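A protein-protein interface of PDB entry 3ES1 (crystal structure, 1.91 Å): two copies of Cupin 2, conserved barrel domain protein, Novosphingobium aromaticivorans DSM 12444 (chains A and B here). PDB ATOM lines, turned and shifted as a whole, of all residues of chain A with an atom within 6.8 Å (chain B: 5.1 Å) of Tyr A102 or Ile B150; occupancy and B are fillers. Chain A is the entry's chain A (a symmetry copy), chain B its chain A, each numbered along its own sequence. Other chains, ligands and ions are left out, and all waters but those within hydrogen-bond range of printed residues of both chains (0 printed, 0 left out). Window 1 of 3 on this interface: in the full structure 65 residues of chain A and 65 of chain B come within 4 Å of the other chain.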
ATOM      1  N   ILE A  81      30.912  11.779  23.883  1.00  0.00           N
ATOM      2  CA  ILE A  81      30.623  11.064  25.143  1.00  0.00           C
ATOM      3  C   ILE A  81      31.489  11.667  26.229  1.00  0.00           C
ATOM      4  O   ILE A  81      32.695  11.763  26.097  1.00  0.00           O
ATOM      5  CB  ILE A  81      30.767   9.490  25.056  1.00  0.00           C
ATOM      6  CG1 ILE A  81      30.454   8.802  26.416  1.00  0.00           C
ATOM      7  CG2 ILE A  81      32.145   9.074  24.542  1.00  0.00           C
ATOM      8  CD1 ILE A  81      30.232   7.284  26.323  1.00  0.00           C
ATOM      9  N   ILE A 100      20.341  14.970  20.136  1.00  0.00           N
ATOM     10  CA  ILE A 100      19.660  13.998  20.996  1.00  0.00           C
ATOM     11  C   ILE A 100      20.745  13.428  21.881  1.00  0.00           C
ATOM     12  O   ILE A 100      21.836  13.152  21.427  1.00  0.00           O
ATOM     13  CB  ILE A 100      18.890  12.885  20.186  1.00  0.00           C
ATOM     14  CG1 ILE A 100      17.960  12.053  21.087  1.00  0.00           C
ATOM     15  CG2 ILE A 100      19.807  11.936  19.346  1.00  0.00           C
ATOM     16  CD1 ILE A 100      17.052  11.047  20.302  1.00  0.00           C
ATOM     17  N   ASP A 101      20.449  13.323  23.164  1.00  0.00           N
ATOM     18  CA  ASP A 101      21.390  12.818  24.134  1.00  0.00           C
ATOM     19  C   ASP A 101      20.875  11.601  24.881  1.00  0.00           C
ATOM     20  O   ASP A 101      19.764  11.579  25.281  1.00  0.00           O
ATOM     21  CB  ASP A 101      21.759  13.864  25.175  1.00  0.00           C
ATOM     22  CG  ASP A 101      21.745  15.257  24.647  1.00  0.00           C
ATOM     23  OD1 ASP A 101      22.338  15.473  23.612  1.00  0.00           O
ATOM     24  OD2 ASP A 101      21.151  16.068  25.315  1.00  0.00           O
ATOM     25  N   TYR A 102      21.714  10.615  25.066  1.00  0.00           N
ATOM     26  CA  TYR A 102      21.428   9.478  25.913  1.00  0.00           C
ATOM     27  C   TYR A 102      22.217   9.684  27.205  1.00  0.00           C
ATOM     28  O   TYR A 102      23.441   9.758  27.201  1.00  0.00           O
ATOM     29  CB  TYR A 102      21.823   8.147  25.255  1.00  0.00           C
ATOM     30  CG  TYR A 102      21.238   7.925  23.911  1.00  0.00           C
ATOM     31  CD1 TYR A 102      19.881   8.237  23.648  1.00  0.00           C
ATOM     32  CD2 TYR A 102      22.015   7.401  22.855  1.00  0.00           C
ATOM     33  CE1 TYR A 102      19.330   8.019  22.374  1.00  0.00           C
ATOM     34  CE2 TYR A 102      21.450   7.189  21.574  1.00  0.00           C
ATOM     35  CZ  TYR A 102      20.094   7.472  21.352  1.00  0.00           C
ATOM     36  OH  TYR A 102      19.551   7.262  20.088  1.00  0.00           O
ATOM     37  N   GLY A 103      21.506   9.774  28.308  1.00  0.00           N
ATOM     38  CA  GLY A 103      22.161   9.918  29.611  1.00  0.00           C
ATOM     39  C   GLY A 103      21.938   8.689  30.451  1.00  0.00           C
ATOM     40  O   GLY A 103      20.813   8.216  30.574  1.00  0.00           O
ATOM     41  N   ILE A 104      23.020   8.196  31.062  1.00  0.00           N
ATOM     42  CA  ILE A 104      22.945   7.005  31.919  1.00  0.00           C
ATOM     43  C   ILE A 104      23.450   7.309  33.299  1.00  0.00           C
ATOM     44  O   ILE A 104      24.616   7.717  33.495  1.00  0.00           O
ATOM     45  CB  ILE A 104      23.691   5.756  31.301  1.00  0.00           C
ATOM     46  CG1 ILE A 104      23.226   5.509  29.837  1.00  0.00           C
ATOM     47  CG2 ILE A 104      23.375   4.486  32.089  1.00  0.00           C
ATOM     48  CD1 ILE A 104      24.117   6.162  28.780  1.00  0.00           C
ATOM     49  N   ILE A 127      18.009   5.699  32.507  1.00  0.00           N
ATOM     50  CA  ILE A 127      18.403   6.310  31.227  1.00  0.00           C
ATOM     51  C   ILE A 127      17.457   7.410  30.775  1.00  0.00           C
ATOM     52  O   ILE A 127      16.229   7.249  30.756  1.00  0.00           O
ATOM     53  CB  ILE A 127      18.530   5.239  30.112  1.00  0.00           C
ATOM     54  CG1 ILE A 127      19.621   4.203  30.499  1.00  0.00           C
ATOM     55  CG2 ILE A 127      18.837   5.897  28.767  1.00  0.00           C
ATOM     56  CD1 ILE A 127      19.714   2.925  29.579  1.00  0.00           C
ATOM     57  N   ILE A 128      18.071   8.524  30.373  1.00  0.00           N
ATOM     58  CA  ILE A 128      17.360   9.662  29.823  1.00  0.00           C
ATOM     59  C   ILE A 128      17.589   9.748  28.307  1.00  0.00           C
ATOM     60  O   ILE A 128      18.716   9.647  27.826  1.00  0.00           O
ATOM     61  CB  ILE A 128      17.774  11.014  30.438  1.00  0.00           C
ATOM     62  CG1 ILE A 128      17.740  10.955  31.992  1.00  0.00           C
ATOM     63  CG2 ILE A 128      16.894  12.104  29.891  1.00  0.00           C
ATOM     64  CD1 ILE A 128      19.124  10.648  32.547  1.00  0.00           C
ATOM     65  N   VAL A 129      16.481   9.898  27.587  1.00  0.00           N
ATOM     66  CA  VAL A 129      16.514  10.238  26.146  1.00  0.00           C
ATOM     67  C   VAL A 129      16.103  11.701  26.008  1.00  0.00           C
ATOM     68  O   VAL A 129      14.916  12.033  26.097  1.00  0.00           O
ATOM     69  CB  VAL A 129      15.595   9.294  25.333  1.00  0.00           C
ATOM     70  CG1 VAL A 129      15.690   9.540  23.824  1.00  0.00           C
ATOM     71  CG2 VAL A 129      15.936   7.806  25.671  1.00  0.00           C
ATOM     72  N   GLN A 130      17.086  12.565  25.816  1.00  0.00           N
ATOM     73  CA  GLN A 130      16.884  14.002  25.801  1.00  0.00           C
ATOM     74  C   GLN A 130      16.728  14.457  24.366  1.00  0.00           C
ATOM     75  O   GLN A 130      17.647  14.479  23.646  1.00  0.00           O
ATOM     76  CB  GLN A 130      18.026  14.753  26.525  1.00  0.00           C
ATOM     77  CG  GLN A 130      17.877  16.241  26.685  1.00  0.00           C
ATOM     78  CD  GLN A 130      17.362  16.629  28.067  1.00  0.00           C
ATOM     79  OE1 GLN A 130      16.287  17.085  28.207  1.00  0.00           O
ATOM     80  NE2 GLN A 130      18.123  16.383  29.048  1.00  0.00           N
ATOM     81  N   ILE A 147      26.863  10.769  35.831  1.00  0.00           N
ATOM     82  CA  ILE A 147      26.084  10.477  34.636  1.00  0.00           C
ATOM     83  C   ILE A 147      26.994  10.432  33.408  1.00  0.00           C
ATOM     84  O   ILE A 147      27.852  11.266  33.226  1.00  0.00           O
ATOM     85  CB  ILE A 147      24.930  11.538  34.391  1.00  0.00           C
ATOM     86  CG1 ILE A 147      24.058  11.728  35.644  1.00  0.00           C
ATOM     87  CG2 ILE A 147      24.039  11.096  33.207  1.00  0.00           C
ATOM     88  CD1 ILE A 147      23.099  12.948  35.604  1.00  0.00           C
ATOM     89  N   ALA A 148      26.817   9.387  32.616  1.00  0.00           N
ATOM     90  CA  ALA A 148      27.471   9.295  31.292  1.00  0.00           C
ATOM     91  C   ALA A 148      26.508   9.851  30.268  1.00  0.00           C
ATOM     92  O   ALA A 148      25.338   9.390  30.161  1.00  0.00           O
ATOM     93  CB  ALA A 148      27.806   7.806  30.945  1.00  0.00           C
ATOM     94  N   PHE A 149      27.000  10.817  29.505  1.00  0.00           N
ATOM     95  CA  PHE A 149      26.217  11.463  28.469  1.00  0.00           C
ATOM     96  C   PHE A 149      26.807  11.238  27.089  1.00  0.00           C
ATOM     97  O   PHE A 149      27.989  11.501  26.830  1.00  0.00           O
ATOM     98  CB  PHE A 149      26.152  12.983  28.677  1.00  0.00           C
ATOM     99  CG  PHE A 149      25.296  13.416  29.810  1.00  0.00           C
ATOM    100  CD1 PHE A 149      23.923  13.290  29.750  1.00  0.00           C
ATOM    101  CD2 PHE A 149      25.859  13.978  30.931  1.00  0.00           C
ATOM    102  CE1 PHE A 149      23.120  13.709  30.814  1.00  0.00           C
ATOM    103  CE2 PHE A 149      25.049  14.428  32.001  1.00  0.00           C
ATOM    104  CZ  PHE A 149      23.697  14.290  31.946  1.00  0.00           C
ATOM    105  N   ILE A 150      25.932  10.805  26.194  1.00  0.00           N
ATOM    106  CA  ILE A 150      26.229  10.705  24.777  1.00  0.00           C
ATOM    107  C   ILE A 150      25.354  11.671  23.969  1.00  0.00           C
ATOM    108  O   ILE A 150      24.140  11.550  23.932  1.00  0.00           O
ATOM    109  CB  ILE A 150      26.040   9.269  24.242  1.00  0.00           C
ATOM    110  CG1 ILE A 150      26.917   8.250  24.999  1.00  0.00           C
ATOM    111  CG2 ILE A 150      26.394   9.190  22.728  1.00  0.00           C
ATOM    112  CD1 ILE A 150      26.391   7.761  26.372  1.00  0.00           C
ATOM    113  N   LEU A 151      25.997  12.613  23.293  1.00  0.00           N
ATOM    114  CA  LEU A 151      25.280  13.644  22.573  1.00  0.00           C
ATOM    115  C   LEU A 151      25.493  13.455  21.086  1.00  0.00           C
ATOM    116  O   LEU A 151      26.606  13.392  20.611  1.00  0.00           O
ATOM    117  CB  LEU A 151      25.706  15.076  23.039  1.00  0.00           C
ATOM    118  CG  LEU A 151      25.573  15.390  24.553  1.00  0.00           C
ATOM    119  CD1 LEU A 151      26.851  15.010  25.361  1.00  0.00           C
ATOM    120  CD2 LEU A 151      25.216  16.870  24.804  1.00  0.00           C
ATOM    121  N   ILE A 152      24.387  13.383  20.358  1.00  0.00           N
ATOM    122  CA  ILE A 152      24.420  13.125  18.925  1.00  0.00           C
ATOM    123  C   ILE A 152      23.708  14.254  18.186  1.00  0.00           C
ATOM    124  O   ILE A 152      22.574  14.607  18.497  1.00  0.00           O
ATOM    125  CB  ILE A 152      23.742  11.762  18.583  1.00  0.00           C
ATOM    126  CG1 ILE A 152      24.469  10.576  19.230  1.00  0.00           C
ATOM    127  CG2 ILE A 152      23.682  11.538  17.052  1.00  0.00           C
ATOM    128  CD1 ILE A 152      23.634   9.293  19.285  1.00  0.00           C
ATOM    129  N   TRP B  51      16.387   2.901  22.923  1.00  0.00           N
ATOM    130  CA  TRP B  51      16.078   3.899  21.891  1.00  0.00           C
ATOM    131  C   TRP B  51      16.861   3.613  20.619  1.00  0.00           C
ATOM    132  O   TRP B  51      17.910   2.948  20.643  1.00  0.00           O
ATOM    133  CB  TRP B  51      16.400   5.342  22.396  1.00  0.00           C
ATOM    134  CG  TRP B  51      15.644   6.450  21.673  1.00  0.00           C
ATOM    135  CD1 TRP B  51      16.098   7.209  20.654  1.00  0.00           C
ATOM    136  CD2 TRP B  51      14.280   6.843  21.881  1.00  0.00           C
ATOM    137  NE1 TRP B  51      15.125   8.058  20.207  1.00  0.00           N
ATOM    138  CE2 TRP B  51      13.995   7.867  20.952  1.00  0.00           C
ATOM    139  CE3 TRP B  51      13.269   6.424  22.754  1.00  0.00           C
ATOM    140  CZ2 TRP B  51      12.733   8.476  20.878  1.00  0.00           C
ATOM    141  CZ3 TRP B  51      12.066   7.024  22.703  1.00  0.00           C
ATOM    142  CH2 TRP B  51      11.787   8.041  21.765  1.00  0.00           C
ATOM    143  N   THR B  52      16.327   4.169  19.544  1.00  0.00           N
ATOM    144  CA  THR B  52      16.947   4.203  18.216  1.00  0.00           C
ATOM    145  C   THR B  52      16.615   5.489  17.508  1.00  0.00           C
ATOM    146  O   THR B  52      15.565   6.086  17.742  1.00  0.00           O
ATOM    147  CB  THR B  52      16.448   3.074  17.312  1.00  0.00           C
ATOM    148  OG1 THR B  52      15.063   3.253  17.018  1.00  0.00           O
ATOM    149  CG2 THR B  52      16.683   1.714  17.976  1.00  0.00           C
ATOM    150  N   THR B  53      17.495   5.912  16.618  1.00  0.00           N
ATOM    151  CA  THR B  53      17.171   6.993  15.660  1.00  0.00           C
ATOM    152  C   THR B  53      17.356   6.431  14.259  1.00  0.00           C
ATOM    153  O   THR B  53      18.275   5.628  14.028  1.00  0.00           O
ATOM    154  CB  THR B  53      18.069   8.243  15.919  1.00  0.00           C
ATOM    155  OG1 THR B  53      19.427   7.947  15.604  1.00  0.00           O
ATOM    156  CG2 THR B  53      17.968   8.665  17.370  1.00  0.00           C
ATOM    157  N   SER B  79      21.306   5.447  15.015  1.00  0.00           N
ATOM    158  CA  SER B  79      21.842   5.095  16.333  1.00  0.00           C
ATOM    159  C   SER B  79      20.936   4.185  17.095  1.00  0.00           C
ATOM    160  O   SER B  79      19.731   4.099  16.858  1.00  0.00           O
ATOM    161  CB  SER B  79      22.182   6.334  17.192  1.00  0.00           C
ATOM    162  OG  SER B  79      21.045   6.990  17.743  1.00  0.00           O
ATOM    163  N   VAL B  80      21.573   3.494  18.016  1.00  0.00           N
ATOM    164  CA  VAL B  80      20.925   2.495  18.909  1.00  0.00           C
ATOM    165  C   VAL B  80      21.489   2.628  20.324  1.00  0.00           C
ATOM    166  O   VAL B  80      22.708   2.720  20.518  1.00  0.00           O
ATOM    167  CB  VAL B  80      21.158   1.028  18.434  1.00  0.00           C
ATOM    168  CG1 VAL B  80      20.540   0.034  19.416  1.00  0.00           C
ATOM    169  CG2 VAL B  80      20.539   0.781  17.049  1.00  0.00           C
ATOM    170  N   ILE B  81      20.617   2.660  21.314  1.00  0.00           N
ATOM    171  CA  ILE B  81      21.071   2.442  22.703  1.00  0.00           C
ATOM    172  C   ILE B  81      20.307   1.260  23.262  1.00  0.00           C
ATOM    173  O   ILE B  81      19.091   1.221  23.233  1.00  0.00           O
ATOM    174  CB  ILE B  81      20.979   3.720  23.633  1.00  0.00           C
ATOM    175  CG1 ILE B  81      21.466   3.420  25.081  1.00  0.00           C
ATOM    176  CG2 ILE B  81      19.569   4.312  23.648  1.00  0.00           C
ATOM    177  CD1 ILE B  81      21.735   4.671  25.931  1.00  0.00           C
ATOM    178  N   ILE B 100      30.579   2.917  15.260  1.00  0.00           N
ATOM    179  CA  ILE B 100      31.388   3.165  16.456  1.00  0.00           C
ATOM    180  C   ILE B 100      30.430   3.017  17.616  1.00  0.00           C
ATOM    181  O   ILE B 100      29.307   3.472  17.558  1.00  0.00           O
ATOM    182  CB  ILE B 100      32.107   4.570  16.439  1.00  0.00           C
ATOM    183  CG1 ILE B 100      33.162   4.692  17.553  1.00  0.00           C
ATOM    184  CG2 ILE B 100      31.139   5.798  16.482  1.00  0.00           C
ATOM    185  CD1 ILE B 100      34.016   6.003  17.474  1.00  0.00           C
ATOM    186  N   ASP B 101      30.869   2.309  18.642  1.00  0.00           N
ATOM    187  CA  ASP B 101      30.061   2.062  19.811  1.00  0.00           C
ATOM    188  C   ASP B 101      30.702   2.565  21.092  1.00  0.00           C
ATOM    189  O   ASP B 101      31.850   2.376  21.293  1.00  0.00           O
ATOM    190  CB  ASP B 101      29.769   0.581  20.004  1.00  0.00           C
ATOM    191  CG  ASP B 101      29.671  -0.177  18.725  1.00  0.00           C
ATOM    192  OD1 ASP B 101      28.959   0.279  17.855  1.00  0.00           O
ATOM    193  OD2 ASP B 101      30.302  -1.203  18.671  1.00  0.00           O
ATOM    194  N   TYR B 102      29.927   3.186  21.942  1.00  0.00           N
ATOM    195  CA  TYR B 102      30.349   3.556  23.276  1.00  0.00           C
ATOM    196  C   TYR B 102      29.699   2.558  24.233  1.00  0.00           C
ATOM    197  O   TYR B 102      28.480   2.457  24.320  1.00  0.00           O
ATOM    198  CB  TYR B 102      29.936   4.990  23.640  1.00  0.00           C
ATOM    199  CG  TYR B 102      30.377   6.025  22.675  1.00  0.00           C
ATOM    200  CD1 TYR B 102      31.684   5.998  22.128  1.00  0.00           C
ATOM    201  CD2 TYR B 102      29.510   7.064  22.270  1.00  0.00           C
ATOM    202  CE1 TYR B 102      32.099   6.985  21.217  1.00  0.00           C
ATOM    203  CE2 TYR B 102      29.938   8.050  21.349  1.00  0.00           C
ATOM    204  CZ  TYR B 102      31.249   8.020  20.852  1.00  0.00           C
ATOM    205  OH  TYR B 102      31.658   8.993  19.946  1.00  0.00           O
ATOM    206  N   GLY B 103      30.523   1.828  24.952  1.00  0.00           N
ATOM    207  CA  GLY B 103      30.011   0.878  25.942  1.00  0.00           C
ATOM    208  C   GLY B 103      30.373   1.320  27.334  1.00  0.00           C
ATOM    209  O   GLY B 103      31.522   1.656  27.601  1.00  0.00           O
ATOM    210  N   ILE B 104      29.384   1.281  28.234  1.00  0.00           N
ATOM    211  CA  ILE B 104      29.600   1.680  29.632  1.00  0.00           C
ATOM    212  C   ILE B 104      29.238   0.562  30.565  1.00  0.00           C
ATOM    213  O   ILE B 104      28.086   0.076  30.591  1.00  0.00           O
ATOM    214  CB  ILE B 104      28.840   3.011  30.016  1.00  0.00           C
ATOM    215  CG1 ILE B 104      29.150   4.136  28.986  1.00  0.00           C
ATOM    216  CG2 ILE B 104      29.289   3.523  31.383  1.00  0.00           C
ATOM    217  CD1 ILE B 104      28.123   4.252  27.860  1.00  0.00           C
ATOM    218  N   ALA B 148      25.739  -0.764  29.111  1.00  0.00           N
ATOM    219  CA  ALA B 148      24.947   0.108  28.217  1.00  0.00           C
ATOM    220  C   ALA B 148      25.769   0.351  26.971  1.00  0.00           C
ATOM    221  O   ALA B 148      26.937   0.823  27.047  1.00  0.00           O
ATOM    222  CB  ALA B 148      24.633   1.473  28.914  1.00  0.00           C
ATOM    223  N   PHE B 149      25.158   0.054  25.832  1.00  0.00           N
ATOM    224  CA  PHE B 149      25.797   0.227  24.541  1.00  0.00           C
ATOM    225  C   PHE B 149      25.067   1.240  23.679  1.00  0.00           C
ATOM    226  O   PHE B 149      23.855   1.151  23.445  1.00  0.00           O
ATOM    227  CB  PHE B 149      25.826  -1.087  23.747  1.00  0.00           C
ATOM    228  CG  PHE B 149      26.784  -2.099  24.259  1.00  0.00           C
ATOM    229  CD1 PHE B 149      28.146  -1.910  24.140  1.00  0.00           C
ATOM    230  CD2 PHE B 149      26.326  -3.259  24.838  1.00  0.00           C
ATOM    231  CE1 PHE B 149      29.045  -2.869  24.614  1.00  0.00           C
ATOM    232  CE2 PHE B 149      27.231  -4.246  25.295  1.00  0.00           C
ATOM    233  CZ  PHE B 149      28.574  -4.052  25.190  1.00  0.00           C
ATOM    234  N   ILE B 150      25.855   2.171  23.160  1.00  0.00           N
ATOM    235  CA  ILE B 150      25.408   3.121  22.159  1.00  0.00           C
ATOM    236  C   ILE B 150      26.151   2.906  20.836  1.00  0.00           C
ATOM    237  O   ILE B 150      27.357   3.071  20.749  1.00  0.00           O
ATOM    238  CB  ILE B 150      25.592   4.583  22.622  1.00  0.00           C
ATOM    239  CG1 ILE B 150      24.845   4.873  23.940  1.00  0.00           C
ATOM    240  CG2 ILE B 150      25.077   5.576  21.539  1.00  0.00           C
ATOM    241  CD1 ILE B 150      25.537   4.417  25.249  1.00  0.00           C
ATOM    242  N   LEU B 151      25.401   2.568  19.796  1.00  0.00           N
ATOM    243  CA  LEU B 151      25.994   2.239  18.517  1.00  0.00           C
ATOM    244  C   LEU B 151      25.625   3.307  17.508  1.00  0.00           C
ATOM    245  O   LEU B 151      24.470   3.610  17.302  1.00  0.00           O
ATOM    246  CB  LEU B 151      25.566   0.815  18.031  1.00  0.00           C
ATOM    247  CG  LEU B 151      25.853  -0.369  18.990  1.00  0.00           C
ATOM    248  CD1 LEU B 151      24.688  -0.628  19.994  1.00  0.00           C
ATOM    249  CD2 LEU B 151      26.178  -1.667  18.223  1.00  0.00           C
ATOM    250  N   ILE B 152      26.646   3.860  16.868  1.00  0.00           N
ATOM    251  CA  ILE B 152      26.466   4.955  15.924  1.00  0.00           C
ATOM    252  C   ILE B 152      27.048   4.562  14.569  1.00  0.00           C
ATOM    253  O   ILE B 152      28.195   4.137  14.464  1.00  0.00           O
ATOM    254  CB  ILE B 152      27.154   6.258  16.434  1.00  0.00           C
ATOM    255  CG1 ILE B 152      26.549   6.752  17.756  1.00  0.00           C
ATOM    256  CG2 ILE B 152      27.055   7.390  15.383  1.00  0.00           C
ATOM    257  CD1 ILE B 152      27.435   7.751  18.507  1.00  0.00           C
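Of the 16 printed residues of chain B, 6 touch a printed residue of chain A.
Printed residues of chain B that touch a printed residue of chain A: Trp B51, Thr B53, Ser B79, Ile B81, Tyr B102 and Ile B150.
Hydrophobic or aromatic side chains of chain A within 4 Å of the printed part of chain B: Ile A81, Ile A100, Tyr A102, Val A129, Ile A150 and Ile A152.
Among the printed residues, 12 pairs touch across the chains.
Among the printed residues, no Asp or Glu carboxylate lies within 4 Å of a Lys or Arg side-chain nitrogen of the other chain.
The side-chain hydroxyl (OH) of Tyr A102 sits at hydrogen-bond distance from the side-chain hydroxyl (OG) of Ser B79, 2.8 Å away.
Tyr A102 touches five residues of chain B.
Of the printed residues of chain B, Ile A150 touches Tyr B102 and Ile B150.
Of the printed residues of chain A, Ser B79 touches Tyr A102 (2.8 Å) and Ile A152 (3.8 Å).
Of the printed residues of chain A, Tyr B102 touches Ile A81 and Ile A150.
Leu B151 touches none of the printed residues of chain A.
Ile A81 touches Tyr B102, and with the chains exchanged Tyr A102 touches Ile B81.
Tyr A102 touches Ile B150, and with the chains exchanged Ile A150 touches Tyr B102.
Ile B150 touches its own counterpart, Ile A150.
Positions printed for both chains: 81, 100, 101, 102, 103, 104, 148, 149, 150, 151 and 152.
Of the 12 pairs that touch across the chains among the printed residues, 5 have their exchanged pair printed and touching as well.
The backbone NH (N) of Ile B81 lies within hydrogen-bond range of the backbone carbonyl oxygen (O) of Trp B51 (2.8 Å).
OG1 of Thr B53 sits at hydrogen-bond distance from OG of Ser B79.
O of Ile B150 lies within hydrogen-bond range of N of Tyr B102, at 2.8 Å.
The backbone carbonyl oxygen of Ile A100 sits at hydrogen-bond distance from the backbone NH of Ile A152.
The backbone carbonyl oxygen (O) of Ile A150 lies within hydrogen-bond range of the backbone NH (N) of Tyr A102 (2.8 Å).
Ile A81 touches Tyr B102 (CD1 to CB, 3.5 Å).
CD1 of Ile A100 touches NE1 of Trp B51, 3.6 Å away.
Thr B53 touches Ile A100 (CG2 to CD1, 3.9 Å).
Tyr A102 touches Trp B51 (OH to CD1, 3.5 Å).
Thr B53 touches Tyr A102.
CB of Tyr A102 touches CD1 of Ile B81, at 3.5 Å.
Ile B150 touches Tyr A102 (CG2 to CD2, 3.8 Å).
CD2 of Trp B51 touches CG1 of Val A129, 3.6 Å away.
Tyr B102 touches Ile A150 (CD2 to CG2, 3.8 Å).
CD1 of Ile A152 touches OG of Ser B79 (3.8 Å).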
